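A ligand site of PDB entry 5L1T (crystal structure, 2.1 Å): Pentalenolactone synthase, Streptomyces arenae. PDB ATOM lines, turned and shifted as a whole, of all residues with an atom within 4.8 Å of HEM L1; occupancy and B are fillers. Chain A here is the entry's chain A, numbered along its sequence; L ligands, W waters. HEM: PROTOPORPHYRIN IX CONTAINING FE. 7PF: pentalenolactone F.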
ATOM      1  N   LEU A  63     -19.952   0.706  11.015  1.00  0.00           N
ATOM      2  CA  LEU A  63     -19.246  -0.555  11.176  1.00  0.00           C
ATOM      3  C   LEU A  63     -18.180  -0.458  12.268  1.00  0.00           C
ATOM      4  O   LEU A  63     -17.986  -1.396  13.039  1.00  0.00           O
ATOM      5  CB  LEU A  63     -18.603  -0.978   9.858  1.00  0.00           C
ATOM      6  CG  LEU A  63     -17.864  -2.317   9.849  1.00  0.00           C
ATOM      7  CD1 LEU A  63     -18.817  -3.470  10.090  1.00  0.00           C
ATOM      8  CD2 LEU A  63     -17.111  -2.516   8.535  1.00  0.00           C
ATOM      9  N   MET A  84     -13.073  -3.754   4.935  1.00  0.00           N
ATOM     10  CA  MET A  84     -14.102  -2.741   4.729  1.00  0.00           C
ATOM     11  C   MET A  84     -13.701  -1.375   5.292  1.00  0.00           C
ATOM     12  O   MET A  84     -14.575  -0.514   5.495  1.00  0.00           O
ATOM     13  CB  MET A  84     -15.419  -3.210   5.356  1.00  0.00           C
ATOM     14  CG  MET A  84     -16.010  -4.453   4.670  1.00  0.00           C
ATOM     15  SD  MET A  84     -17.373  -5.257   5.560  1.00  0.00           S
ATOM     16  CE  MET A  84     -18.718  -4.115   5.264  1.00  0.00           C
ATOM     17  N   HIS A  96     -13.362   4.877   4.020  1.00  0.00           N
ATOM     18  CA  HIS A  96     -14.488   4.144   3.434  1.00  0.00           C
ATOM     19  C   HIS A  96     -15.093   4.893   2.249  1.00  0.00           C
ATOM     20  O   HIS A  96     -15.528   4.255   1.279  1.00  0.00           O
ATOM     21  CB  HIS A  96     -15.564   3.884   4.493  1.00  0.00           C
ATOM     22  CG  HIS A  96     -16.825   3.260   3.940  1.00  0.00           C
ATOM     23  ND1 HIS A  96     -18.027   3.937   3.909  1.00  0.00           N
ATOM     24  CD2 HIS A  96     -17.062   2.033   3.402  1.00  0.00           C
ATOM     25  CE1 HIS A  96     -18.953   3.155   3.394  1.00  0.00           C
ATOM     26  NE2 HIS A  96     -18.390   2.003   3.068  1.00  0.00           N
ATOM     27  N   MET A  99     -12.761   4.010  -0.525  1.00  0.00           N
ATOM     28  CA  MET A  99     -12.973   2.628  -0.926  1.00  0.00           C
ATOM     29  C   MET A  99     -14.116   2.511  -1.919  1.00  0.00           C
ATOM     30  O   MET A  99     -13.972   1.915  -2.991  1.00  0.00           O
ATOM     31  CB  MET A  99     -13.225   1.744   0.300  1.00  0.00           C
ATOM     32  CG  MET A  99     -13.479   0.299  -0.066  1.00  0.00           C
ATOM     33  SD  MET A  99     -14.026  -0.717   1.322  1.00  0.00           S
ATOM     34  CE  MET A  99     -14.269  -2.303   0.521  1.00  0.00           C
ATOM     35  N   ARG A 100     -15.265   3.111  -1.583  1.00  0.00           N
ATOM     36  CA  ARG A 100     -16.420   3.009  -2.473  1.00  0.00           C
ATOM     37  C   ARG A 100     -16.191   3.785  -3.764  1.00  0.00           C
ATOM     38  O   ARG A 100     -16.556   3.308  -4.848  1.00  0.00           O
ATOM     39  CB  ARG A 100     -17.668   3.490  -1.746  1.00  0.00           C
ATOM     40  CG  ARG A 100     -18.084   2.506  -0.631  1.00  0.00           C
ATOM     41  CD  ARG A 100     -19.457   2.793  -0.074  1.00  0.00           C
ATOM     42  NE  ARG A 100     -20.551   2.624  -1.039  1.00  0.00           N
ATOM     43  CZ  ARG A 100     -21.214   1.491  -1.264  1.00  0.00           C
ATOM     44  NH1 ARG A 100     -20.887   0.373  -0.608  1.00  0.00           N
ATOM     45  NH2 ARG A 100     -22.204   1.466  -2.142  1.00  0.00           N
ATOM     46  N   LEU A 103     -14.140   1.501  -6.014  1.00  0.00           N
ATOM     47  CA  LEU A 103     -14.664   0.204  -6.449  1.00  0.00           C
ATOM     48  C   LEU A 103     -15.904   0.333  -7.341  1.00  0.00           C
ATOM     49  O   LEU A 103     -16.076  -0.447  -8.282  1.00  0.00           O
ATOM     50  CB  LEU A 103     -14.993  -0.686  -5.249  1.00  0.00           C
ATOM     51  CG  LEU A 103     -13.845  -1.259  -4.411  1.00  0.00           C
ATOM     52  CD1 LEU A 103     -14.352  -1.941  -3.141  1.00  0.00           C
ATOM     53  CD2 LEU A 103     -13.000  -2.206  -5.264  1.00  0.00           C
ATOM     54  N   PHE A 107     -17.466  -1.658 -11.751  1.00  0.00           N
ATOM     55  CA  PHE A 107     -18.602  -2.476 -12.151  1.00  0.00           C
ATOM     56  C   PHE A 107     -19.490  -1.655 -13.077  1.00  0.00           C
ATOM     57  O   PHE A 107     -20.682  -1.486 -12.815  1.00  0.00           O
ATOM     58  CB  PHE A 107     -19.349  -2.977 -10.920  1.00  0.00           C
ATOM     59  CG  PHE A 107     -18.483  -3.825  -9.987  1.00  0.00           C
ATOM     60  CD1 PHE A 107     -17.649  -3.229  -9.044  1.00  0.00           C
ATOM     61  CD2 PHE A 107     -18.529  -5.229 -10.058  1.00  0.00           C
ATOM     62  CE1 PHE A 107     -16.858  -3.999  -8.188  1.00  0.00           C
ATOM     63  CE2 PHE A 107     -17.740  -6.000  -9.212  1.00  0.00           C
ATOM     64  CZ  PHE A 107     -16.886  -5.388  -8.285  1.00  0.00           C
ATOM     65  N   LEU A 155     -12.951 -10.795 -13.248  1.00  0.00           N
ATOM     66  CA  LEU A 155     -12.723  -9.478 -12.647  1.00  0.00           C
ATOM     67  C   LEU A 155     -11.244  -9.205 -12.431  1.00  0.00           C
ATOM     68  O   LEU A 155     -10.768  -8.098 -12.680  1.00  0.00           O
ATOM     69  CB  LEU A 155     -13.484  -9.358 -11.323  1.00  0.00           C
ATOM     70  CG  LEU A 155     -15.017  -9.346 -11.337  1.00  0.00           C
ATOM     71  CD1 LEU A 155     -15.562  -9.264  -9.925  1.00  0.00           C
ATOM     72  CD2 LEU A 155     -15.544  -8.193 -12.175  1.00  0.00           C
ATOM     73  N   VAL A 232     -12.303  -7.650  -3.215  1.00  0.00           N
ATOM     74  CA  VAL A 232     -12.996  -8.245  -4.347  1.00  0.00           C
ATOM     75  C   VAL A 232     -12.894  -9.778  -4.297  1.00  0.00           C
ATOM     76  O   VAL A 232     -13.882 -10.484  -4.512  1.00  0.00           O
ATOM     77  CB  VAL A 232     -12.456  -7.698  -5.689  1.00  0.00           C
ATOM     78  CG1 VAL A 232     -12.967  -8.545  -6.836  1.00  0.00           C
ATOM     79  CG2 VAL A 232     -12.838  -6.238  -5.883  1.00  0.00           C
ATOM     80  N   PHE A 235     -14.868 -11.043  -0.814  1.00  0.00           N
ATOM     81  CA  PHE A 235     -16.310 -10.804  -0.810  1.00  0.00           C
ATOM     82  C   PHE A 235     -16.982 -11.222  -2.121  1.00  0.00           C
ATOM     83  O   PHE A 235     -18.208 -11.306  -2.181  1.00  0.00           O
ATOM     84  CB  PHE A 235     -16.614  -9.314  -0.572  1.00  0.00           C
ATOM     85  CG  PHE A 235     -16.101  -8.779   0.744  1.00  0.00           C
ATOM     86  CD1 PHE A 235     -15.740  -9.626   1.770  1.00  0.00           C
ATOM     87  CD2 PHE A 235     -15.947  -7.409   0.933  1.00  0.00           C
ATOM     88  CE1 PHE A 235     -15.269  -9.131   2.987  1.00  0.00           C
ATOM     89  CE2 PHE A 235     -15.462  -6.903   2.165  1.00  0.00           C
ATOM     90  CZ  PHE A 235     -15.126  -7.771   3.178  1.00  0.00           C
ATOM     91  N   GLY A 236     -16.201 -11.461  -3.180  1.00  0.00           N
ATOM     92  CA  GLY A 236     -16.770 -11.496  -4.514  1.00  0.00           C
ATOM     93  C   GLY A 236     -17.235 -12.842  -5.047  1.00  0.00           C
ATOM     94  O   GLY A 236     -17.814 -12.865  -6.145  1.00  0.00           O
ATOM     95  N   THR A 239     -20.256 -15.645  -1.003  1.00  0.00           N
ATOM     96  CA  THR A 239     -21.670 -15.438  -0.694  1.00  0.00           C
ATOM     97  C   THR A 239     -22.546 -15.741  -1.899  1.00  0.00           C
ATOM     98  O   THR A 239     -23.711 -16.155  -1.737  1.00  0.00           O
ATOM     99  CB  THR A 239     -21.937 -14.007  -0.200  1.00  0.00           C
ATOM    100  OG1 THR A 239     -21.524 -13.056  -1.187  1.00  0.00           O
ATOM    101  CG2 THR A 239     -21.197 -13.707   1.112  1.00  0.00           C
ATOM    102  N   THR A 240     -22.034 -15.529  -3.115  1.00  0.00           N
ATOM    103  CA  THR A 240     -22.820 -15.889  -4.298  1.00  0.00           C
ATOM    104  C   THR A 240     -22.967 -17.400  -4.410  1.00  0.00           C
ATOM    105  O   THR A 240     -24.055 -17.909  -4.743  1.00  0.00           O
ATOM    106  CB  THR A 240     -22.153 -15.333  -5.562  1.00  0.00           C
ATOM    107  OG1 THR A 240     -21.949 -13.931  -5.397  1.00  0.00           O
ATOM    108  CG2 THR A 240     -23.036 -15.578  -6.793  1.00  0.00           C
ATOM    109  N   ARG A 243     -25.766 -18.417  -2.216  1.00  0.00           N
ATOM    110  CA  ARG A 243     -27.113 -18.104  -2.720  1.00  0.00           C
ATOM    111  C   ARG A 243     -27.539 -19.057  -3.839  1.00  0.00           C
ATOM    112  O   ARG A 243     -28.739 -19.336  -3.973  1.00  0.00           O
ATOM    113  CB  ARG A 243     -27.197 -16.651  -3.204  1.00  0.00           C
ATOM    114  CG  ARG A 243     -26.896 -15.664  -2.066  1.00  0.00           C
ATOM    115  CD  ARG A 243     -27.615 -16.099  -0.776  1.00  0.00           C
ATOM    116  NE  ARG A 243     -27.529 -15.203   0.362  1.00  0.00           N
ATOM    117  CZ  ARG A 243     -26.463 -15.078   1.133  1.00  0.00           C
ATOM    118  NH1 ARG A 243     -25.351 -15.765   0.885  1.00  0.00           N
ATOM    119  NH2 ARG A 243     -26.494 -14.264   2.179  1.00  0.00           N
ATOM    120  N   LEU A 276     -33.095 -14.279  -2.782  1.00  0.00           N
ATOM    121  CA  LEU A 276     -32.320 -13.402  -1.903  1.00  0.00           C
ATOM    122  C   LEU A 276     -33.085 -13.076  -0.633  1.00  0.00           C
ATOM    123  O   LEU A 276     -32.504 -13.023   0.462  1.00  0.00           O
ATOM    124  CB  LEU A 276     -31.927 -12.112  -2.650  1.00  0.00           C
ATOM    125  CG  LEU A 276     -31.036 -12.302  -3.878  1.00  0.00           C
ATOM    126  CD1 LEU A 276     -31.012 -11.075  -4.826  1.00  0.00           C
ATOM    127  CD2 LEU A 276     -29.652 -12.738  -3.427  1.00  0.00           C
ATOM    128  N   ILE A 289     -26.364  -7.771  10.151  1.00  0.00           N
ATOM    129  CA  ILE A 289     -25.388  -6.742   9.829  1.00  0.00           C
ATOM    130  C   ILE A 289     -24.954  -6.089  11.135  1.00  0.00           C
ATOM    131  O   ILE A 289     -25.810  -5.518  11.830  1.00  0.00           O
ATOM    132  CB  ILE A 289     -25.943  -5.698   8.846  1.00  0.00           C
ATOM    133  CG1 ILE A 289     -26.143  -6.333   7.463  1.00  0.00           C
ATOM    134  CG2 ILE A 289     -25.005  -4.508   8.788  1.00  0.00           C
ATOM    135  CD1 ILE A 289     -26.571  -5.320   6.409  1.00  0.00           C
ATOM    136  N   ARG A 291     -23.175  -3.398  13.765  1.00  0.00           N
ATOM    137  CA  ARG A 291     -22.892  -1.967  13.830  1.00  0.00           C
ATOM    138  C   ARG A 291     -22.579  -1.578  15.272  1.00  0.00           C
ATOM    139  O   ARG A 291     -22.816  -2.341  16.204  1.00  0.00           O
ATOM    140  CB  ARG A 291     -24.066  -1.124  13.313  1.00  0.00           C
ATOM    141  CG  ARG A 291     -24.405  -1.315  11.821  1.00  0.00           C
ATOM    142  CD  ARG A 291     -23.360  -0.621  10.942  1.00  0.00           C
ATOM    143  NE  ARG A 291     -23.688  -0.633   9.509  1.00  0.00           N
ATOM    144  CZ  ARG A 291     -23.227  -1.506   8.626  1.00  0.00           C
ATOM    145  NH1 ARG A 291     -22.403  -2.488   8.989  1.00  0.00           N
ATOM    146  NH2 ARG A 291     -23.587  -1.393   7.338  1.00  0.00           N
ATOM    147  N   ILE A 314     -31.212  -8.423   8.893  1.00  0.00           N
ATOM    148  CA  ILE A 314     -31.746  -8.303   7.535  1.00  0.00           C
ATOM    149  C   ILE A 314     -32.524  -9.560   7.141  1.00  0.00           C
ATOM    150  O   ILE A 314     -33.511  -9.477   6.392  1.00  0.00           O
ATOM    151  CB  ILE A 314     -30.611  -7.969   6.538  1.00  0.00           C
ATOM    152  CG1 ILE A 314     -29.522  -9.055   6.546  1.00  0.00           C
ATOM    153  CG2 ILE A 314     -30.018  -6.567   6.825  1.00  0.00           C
ATOM    154  CD1 ILE A 314     -28.388  -8.803   5.539  1.00  0.00           C
ATOM    155  N   ALA A 342     -31.313  -8.047   1.589  1.00  0.00           N
ATOM    156  CA  ALA A 342     -30.243  -9.046   1.550  1.00  0.00           C
ATOM    157  C   ALA A 342     -28.899  -8.488   1.081  1.00  0.00           C
ATOM    158  O   ALA A 342     -27.866  -9.083   1.380  1.00  0.00           O
ATOM    159  CB  ALA A 342     -30.630 -10.227   0.645  1.00  0.00           C
ATOM    160  N   PHE A 343     -28.886  -7.384   0.334  1.00  0.00           N
ATOM    161  CA  PHE A 343     -27.643  -6.676   0.000  1.00  0.00           C
ATOM    162  C   PHE A 343     -27.385  -5.490   0.928  1.00  0.00           C
ATOM    163  O   PHE A 343     -26.518  -4.649   0.638  1.00  0.00           O
ATOM    164  CB  PHE A 343     -27.680  -6.181  -1.454  1.00  0.00           C
ATOM    165  CG  PHE A 343     -27.714  -7.273  -2.507  1.00  0.00           C
ATOM    166  CD1 PHE A 343     -26.687  -8.205  -2.607  1.00  0.00           C
ATOM    167  CD2 PHE A 343     -28.757  -7.330  -3.433  1.00  0.00           C
ATOM    168  CE1 PHE A 343     -26.696  -9.180  -3.596  1.00  0.00           C
ATOM    169  CE2 PHE A 343     -28.779  -8.314  -4.429  1.00  0.00           C
ATOM    170  CZ  PHE A 343     -27.758  -9.243  -4.508  1.00  0.00           C
ATOM    171  N   GLY A 344     -28.124  -5.382   2.025  1.00  0.00           N
ATOM    172  CA  GLY A 344     -27.995  -4.225   2.878  1.00  0.00           C
ATOM    173  C   GLY A 344     -28.668  -2.996   2.273  1.00  0.00           C
ATOM    174  O   GLY A 344     -29.550  -3.079   1.413  1.00  0.00           O
ATOM    175  N   ALA A 347     -25.126   3.367   3.467  1.00  0.00           N
ATOM    176  CA  ALA A 347     -23.742   3.727   3.128  1.00  0.00           C
ATOM    177  C   ALA A 347     -22.915   2.537   2.634  1.00  0.00           C
ATOM    178  O   ALA A 347     -22.037   2.714   1.795  1.00  0.00           O
ATOM    179  CB  ALA A 347     -23.040   4.390   4.322  1.00  0.00           C
ATOM    180  N   ARG A 348     -23.178   1.322   3.133  1.00  0.00           N
ATOM    181  CA  ARG A 348     -22.379   0.152   2.765  1.00  0.00           C
ATOM    182  C   ARG A 348     -23.130  -0.841   1.865  1.00  0.00           C
ATOM    183  O   ARG A 348     -22.687  -1.996   1.735  1.00  0.00           O
ATOM    184  CB  ARG A 348     -21.852  -0.570   4.012  1.00  0.00           C
ATOM    185  CG  ARG A 348     -20.936   0.321   4.874  1.00  0.00           C
ATOM    186  CD  ARG A 348     -20.270  -0.458   6.020  1.00  0.00           C
ATOM    187  NE  ARG A 348     -19.209   0.329   6.663  1.00  0.00           N
ATOM    188  CZ  ARG A 348     -17.926   0.290   6.307  1.00  0.00           C
ATOM    189  NH1 ARG A 348     -17.547  -0.500   5.306  1.00  0.00           N
ATOM    190  NH2 ARG A 348     -17.027   1.029   6.934  1.00  0.00           N
ATOM    191  N   HIS A 349     -24.221  -0.419   1.228  1.00  0.00           N
ATOM    192  CA  HIS A 349     -24.972  -1.182   0.229  1.00  0.00           C
ATOM    193  C   HIS A 349     -24.038  -1.936  -0.715  1.00  0.00           C
ATOM    194  O   HIS A 349     -23.132  -1.345  -1.321  1.00  0.00           O
ATOM    195  CB  HIS A 349     -25.863  -0.222  -0.569  1.00  0.00           C
ATOM    196  CG  HIS A 349     -27.068  -0.871  -1.191  1.00  0.00           C
ATOM    197  ND1 HIS A 349     -28.006  -0.160  -1.911  1.00  0.00           N
ATOM    198  CD2 HIS A 349     -27.489  -2.161  -1.207  1.00  0.00           C
ATOM    199  CE1 HIS A 349     -28.942  -0.980  -2.337  1.00  0.00           C
ATOM    200  NE2 HIS A 349     -28.659  -2.198  -1.928  1.00  0.00           N
ATOM    201  N   CYS A 350     -24.267  -3.250  -0.845  1.00  0.00           N
ATOM    202  CA  CYS A 350     -23.335  -4.159  -1.514  1.00  0.00           C
ATOM    203  C   CYS A 350     -22.890  -3.625  -2.868  1.00  0.00           C
ATOM    204  O   CYS A 350     -23.721  -3.286  -3.716  1.00  0.00           O
ATOM    205  CB  CYS A 350     -23.978  -5.532  -1.694  1.00  0.00           C
ATOM    206  SG  CYS A 350     -23.211  -6.519  -2.978  1.00  0.00           S
ATOM    207  N   ILE A 351     -21.573  -3.523  -3.062  1.00  0.00           N
ATOM    208  CA  ILE A 351     -21.036  -2.973  -4.301  1.00  0.00           C
ATOM    209  C   ILE A 351     -21.229  -3.936  -5.483  1.00  0.00           C
ATOM    210  O   ILE A 351     -21.384  -3.499  -6.632  1.00  0.00           O
ATOM    211  CB  ILE A 351     -19.562  -2.576  -4.078  1.00  0.00           C
ATOM    212  CG1 ILE A 351     -19.495  -1.277  -3.272  1.00  0.00           C
ATOM    213  CG2 ILE A 351     -18.806  -2.401  -5.396  1.00  0.00           C
ATOM    214  CD1 ILE A 351     -18.101  -0.848  -2.945  1.00  0.00           C
ATOM    215  N   GLY A 352     -21.270  -5.237  -5.240  1.00  0.00           N
ATOM    216  CA  GLY A 352     -21.376  -6.195  -6.325  1.00  0.00           C
ATOM    217  C   GLY A 352     -22.776  -6.674  -6.655  1.00  0.00           C
ATOM    218  O   GLY A 352     -22.932  -7.591  -7.470  1.00  0.00           O
ATOM    219  N   LEU A 355     -23.904  -7.371 -10.264  1.00  0.00           N
ATOM    220  CA  LEU A 355     -23.227  -8.534 -10.815  1.00  0.00           C
ATOM    221  C   LEU A 355     -23.755  -9.829 -10.196  1.00  0.00           C
ATOM    222  O   LEU A 355     -23.943 -10.829 -10.903  1.00  0.00           O
ATOM    223  CB  LEU A 355     -21.714  -8.387 -10.611  1.00  0.00           C
ATOM    224  CG  LEU A 355     -20.842  -9.549 -11.096  1.00  0.00           C
ATOM    225  CD1 LEU A 355     -21.018  -9.726 -12.598  1.00  0.00           C
ATOM    226  CD2 LEU A 355     -19.382  -9.295 -10.740  1.00  0.00           C
ATOM    227  N   ALA A 356     -23.991  -9.841  -8.881  1.00  0.00           N
ATOM    228  CA  ALA A 356     -24.529 -11.028  -8.222  1.00  0.00           C
ATOM    229  C   ALA A 356     -25.895 -11.390  -8.786  1.00  0.00           C
ATOM    230  O   ALA A 356     -26.208 -12.580  -8.956  1.00  0.00           O
ATOM    231  CB  ALA A 356     -24.613 -10.806  -6.717  1.00  0.00           C
ATOM    232  N   GLU A 359     -25.444 -13.148 -12.163  1.00  0.00           N
ATOM    233  CA  GLU A 359     -25.042 -14.545 -12.011  1.00  0.00           C
ATOM    234  C   GLU A 359     -26.228 -15.416 -11.648  1.00  0.00           C
ATOM    235  O   GLU A 359     -26.426 -16.492 -12.242  1.00  0.00           O
ATOM    236  CB  GLU A 359     -23.973 -14.671 -10.925  1.00  0.00           C
ATOM    237  CG  GLU A 359     -22.644 -14.037 -11.297  1.00  0.00           C
ATOM    238  CD  GLU A 359     -21.576 -14.336 -10.282  1.00  0.00           C
ATOM    239  OE1 GLU A 359     -20.975 -13.361  -9.771  1.00  0.00           O
ATOM    240  OE2 GLU A 359     -21.365 -15.528  -9.955  1.00  0.00           O
ATOM    241  N   LEU A 360     -27.019 -14.984 -10.662  1.00  0.00           N
ATOM    242  CA  LEU A 360     -28.131 -15.774 -10.168  1.00  0.00           C
ATOM    243  C   LEU A 360     -29.241 -15.881 -11.210  1.00  0.00           C
ATOM    244  O   LEU A 360     -29.837 -16.953 -11.382  1.00  0.00           O
ATOM    245  CB  LEU A 360     -28.652 -15.171  -8.853  1.00  0.00           C
ATOM    246  CG  LEU A 360     -27.759 -15.218  -7.600  1.00  0.00           C
ATOM    247  CD1 LEU A 360     -28.398 -14.452  -6.436  1.00  0.00           C
ATOM    248  CD2 LEU A 360     -27.414 -16.660  -7.156  1.00  0.00           C
HETATM  249  CHA HEM L   1     -21.199  -5.436   1.108  1.00  0.00           C
HETATM  250  CHB HEM L   1     -24.281  -9.174   0.605  1.00  0.00           C
HETATM  251  CHC HEM L   1     -22.085 -10.442  -3.532  1.00  0.00           C
HETATM  252  CHD HEM L   1     -18.800  -6.908  -2.899  1.00  0.00           C
HETATM  253  C1A HEM L   1     -22.262  -6.287   1.334  1.00  0.00           C
HETATM  254  C2A HEM L   1     -23.276  -6.199   2.392  1.00  0.00           C
HETATM  255  C3A HEM L   1     -24.112  -7.247   2.230  1.00  0.00           C
HETATM  256  C4A HEM L   1     -23.675  -8.022   1.083  1.00  0.00           C
HETATM  257  CMA HEM L   1     -25.341  -7.598   3.113  1.00  0.00           C
HETATM  258  CAA HEM L   1     -23.387  -5.097   3.490  1.00  0.00           C
HETATM  259  CBA HEM L   1     -22.422  -5.293   4.666  1.00  0.00           C
HETATM  260  CGA HEM L   1     -22.635  -4.217   5.724  1.00  0.00           C
HETATM  261  O1A HEM L   1     -23.562  -3.369   5.570  1.00  0.00           O
HETATM  262  O2A HEM L   1     -21.887  -4.200   6.741  1.00  0.00           O
HETATM  263  C1B HEM L   1     -23.981  -9.859  -0.568  1.00  0.00           C
HETATM  264  C2B HEM L   1     -24.711 -10.990  -1.128  1.00  0.00           C
HETATM  265  C3B HEM L   1     -24.090 -11.346  -2.266  1.00  0.00           C
HETATM  266  C4B HEM L   1     -22.965 -10.437  -2.469  1.00  0.00           C
HETATM  267  CMB HEM L   1     -25.953 -11.645  -0.473  1.00  0.00           C
HETATM  268  CAB HEM L   1     -24.447 -12.473  -3.275  1.00  0.00           C
HETATM  269  CBB HEM L   1     -25.706 -12.897  -3.473  1.00  0.00           C
HETATM  270  C1C HEM L   1     -21.017  -9.578  -3.739  1.00  0.00           C
HETATM  271  C2C HEM L   1     -20.155  -9.603  -4.889  1.00  0.00           C
HETATM  272  C3C HEM L   1     -19.226  -8.627  -4.736  1.00  0.00           C
HETATM  273  C4C HEM L   1     -19.490  -7.962  -3.455  1.00  0.00           C
HETATM  274  CMC HEM L   1     -20.343 -10.617  -6.066  1.00  0.00           C
HETATM  275  CAC HEM L   1     -18.061  -8.225  -5.665  1.00  0.00           C
HETATM  276  CBC HEM L   1     -17.607  -8.973  -6.674  1.00  0.00           C
HETATM  277  C1D HEM L   1     -19.123  -6.232  -1.731  1.00  0.00           C
HETATM  278  C2D HEM L   1     -18.348  -5.203  -1.075  1.00  0.00           C
HETATM  279  C3D HEM L   1     -19.000  -4.808   0.033  1.00  0.00           C
HETATM  280  C4D HEM L   1     -20.217  -5.570   0.134  1.00  0.00           C
HETATM  281  CMD HEM L   1     -16.982  -4.681  -1.573  1.00  0.00           C
HETATM  282  CAD HEM L   1     -18.536  -3.722   1.038  1.00  0.00           C
HETATM  283  CBD HEM L   1     -19.286  -2.429   0.778  1.00  0.00           C
HETATM  284  CGD HEM L   1     -18.945  -1.352   1.785  1.00  0.00           C
HETATM  285  O1D HEM L   1     -19.174  -0.156   1.471  1.00  0.00           O
HETATM  286  O2D HEM L   1     -18.455  -1.692   2.912  1.00  0.00           O
HETATM  287  NA  HEM L   1     -22.557  -7.399   0.557  1.00  0.00           N
HETATM  288  NB  HEM L   1     -22.937  -9.557  -1.421  1.00  0.00           N
HETATM  289  NC  HEM L   1     -20.579  -8.581  -2.884  1.00  0.00           N
HETATM  290  ND  HEM L   1     -20.261  -6.425  -0.965  1.00  0.00           N
HETATM  291 FE   HEM L   1     -21.729  -7.837  -1.346  1.00  0.00          FE
HETATM  292  C1  7PF L   2     -21.243  -9.098   3.146  1.00  0.00           C
HETATM  293  C2  7PF L   2     -19.862  -9.359   3.761  1.00  0.00           C
HETATM  294  C15 7PF L   2     -18.946  -8.179   3.462  1.00  0.00           C
HETATM  295  C14 7PF L   2     -19.202 -10.635   3.186  1.00  0.00           C
HETATM  296  C7  7PF L   2     -23.041 -10.804   3.731  1.00  0.00           C
HETATM  297  C12 7PF L   2     -21.960 -12.193   6.654  1.00  0.00           C
HETATM  298  C10 7PF L   2     -23.771  -9.386   6.719  1.00  0.00           C
HETATM  299  C3  7PF L   2     -20.181  -9.408   5.269  1.00  0.00           C
HETATM  300  C13 7PF L   2     -23.109 -13.175   4.137  1.00  0.00           C
HETATM  301  C11 7PF L   2     -21.643 -10.115   7.845  1.00  0.00           C
HETATM  302  C6  7PF L   2     -22.562 -11.934   4.329  1.00  0.00           C
HETATM  303  C8  7PF L   2     -22.330  -9.629   4.147  1.00  0.00           C
HETATM  304  C5  7PF L   2     -21.535 -11.610   5.268  1.00  0.00           C
HETATM  305  C9  7PF L   2     -22.280  -9.612   6.695  1.00  0.00           C
HETATM  306  C4  7PF L   2     -21.569 -10.090   5.392  1.00  0.00           C
HETATM  307  O4  7PF L   2     -24.113 -13.342   3.400  1.00  0.00           O
HETATM  308  O2  7PF L   2     -21.295  -9.356   8.756  1.00  0.00           O
HETATM  309  O5  7PF L   2     -22.617 -14.219   4.630  1.00  0.00           O
HETATM  310  O3  7PF L   2     -21.388 -11.470   7.825  1.00  0.00           O
HETATM  311  O1  7PF L   2     -22.799  -8.289   6.748  1.00  0.00           O
HETATM  312  O   HOH W   1     -20.140 -13.343  -3.529  1.00  0.00           O
HETATM  313  O   HOH W   2     -25.432  -2.186   4.087  1.00  0.00           O
HETATM  314  O   HOH W   3     -20.755  -6.378   7.997  1.00  0.00           O
HETATM  315  O   HOH W   4     -20.152 -10.791  -0.347  1.00  0.00           O
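SG of Cys 350 binds FE of HEM L1.
NH2 of Arg 291 lies within salt-bridge range of O1A of HEM L1, at 2.7 Å.
The guanidinium group of Arg 100 lies within salt-bridge range of an oxygen (O1D) of HEM L1.
NE2 of His 96 is in hydrogen-bond range of O1D of HEM L1, at 2.8 Å.
O2D of HEM L1 lies within salt-bridge range of NH1 of Arg 348, 2.8 Å away.
NH2 of Arg 243 lies within salt-bridge range of O4 of 7PF L2 (2.8 Å).
SG of Cys 350 lies close to N of Gly 352 (3.2 Å).
N of Cys 350 is in hydrogen-bond range of O of Phe 343.
The backbone carbonyl oxygen (O) of Ala 347 lies close to the guanidinium group (NE) of Arg 100, 3.2 Å away.
The guanidinium group (NH1) of Arg 100 lies within hydrogen-bond range of the backbone carbonyl oxygen (O) of His 349 (2.9 Å).
A ring nitrogen (NE2) of His 96 sits close to the guanidinium group (NH1) of Arg 348, at 3.5 Å.
The guanidinium group (NH1) of Arg 348 lies within hydrogen-bond range of the backbone carbonyl oxygen (O) of Met 84 (3.0 Å).
O of Thr 239 sits at hydrogen-bond distance from NH1 of Arg 243 (3.1 Å).
Residues that only touch HEM L1: Thr 239 (3.3 Å), Arg 243 (3.3 Å), Gly 236 (3.4 Å), Met 84 (3.4 Å), Ala 342 (3.4 Å), Thr 240 (3.6 Å), Gly 352 (3.6 Å), Phe 343 (3.6 Å), Phe 235 (3.6 Å), Ile 289 (3.7 Å), Gly 344 (3.7 Å), Ile 351 (3.8 Å), Ala 356 (3.8 Å), Leu 155 (3.9 Å), Phe 107 (3.9 Å) and Leu 276 (3.9 Å).
Hydrophobic or aromatic side chains within 4 Å of HEM L1: Met 84, His 96, Phe 107, Leu 155, Phe 235, Leu 276, Ile 289, Phe 343 and Ala 356.
Of the 31 residues printed, 21 come within 4 Å of HEM L1.
Water W3 lies within hydrogen-bond range of an oxygen (O2A) of HEM L1 and an oxygen (O1) of 7PF L2.
Water W4 lies within hydrogen-bond range of the backbone carbonyl oxygen of Phe 235 and the side-chain hydroxyl of Thr 239.
Water W1 lies within hydrogen-bond range of OG1 of Thr 240 (2.7 Å), OG1 of Thr 239 (2.7 Å) and O of Phe 235 (3.1 Å).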
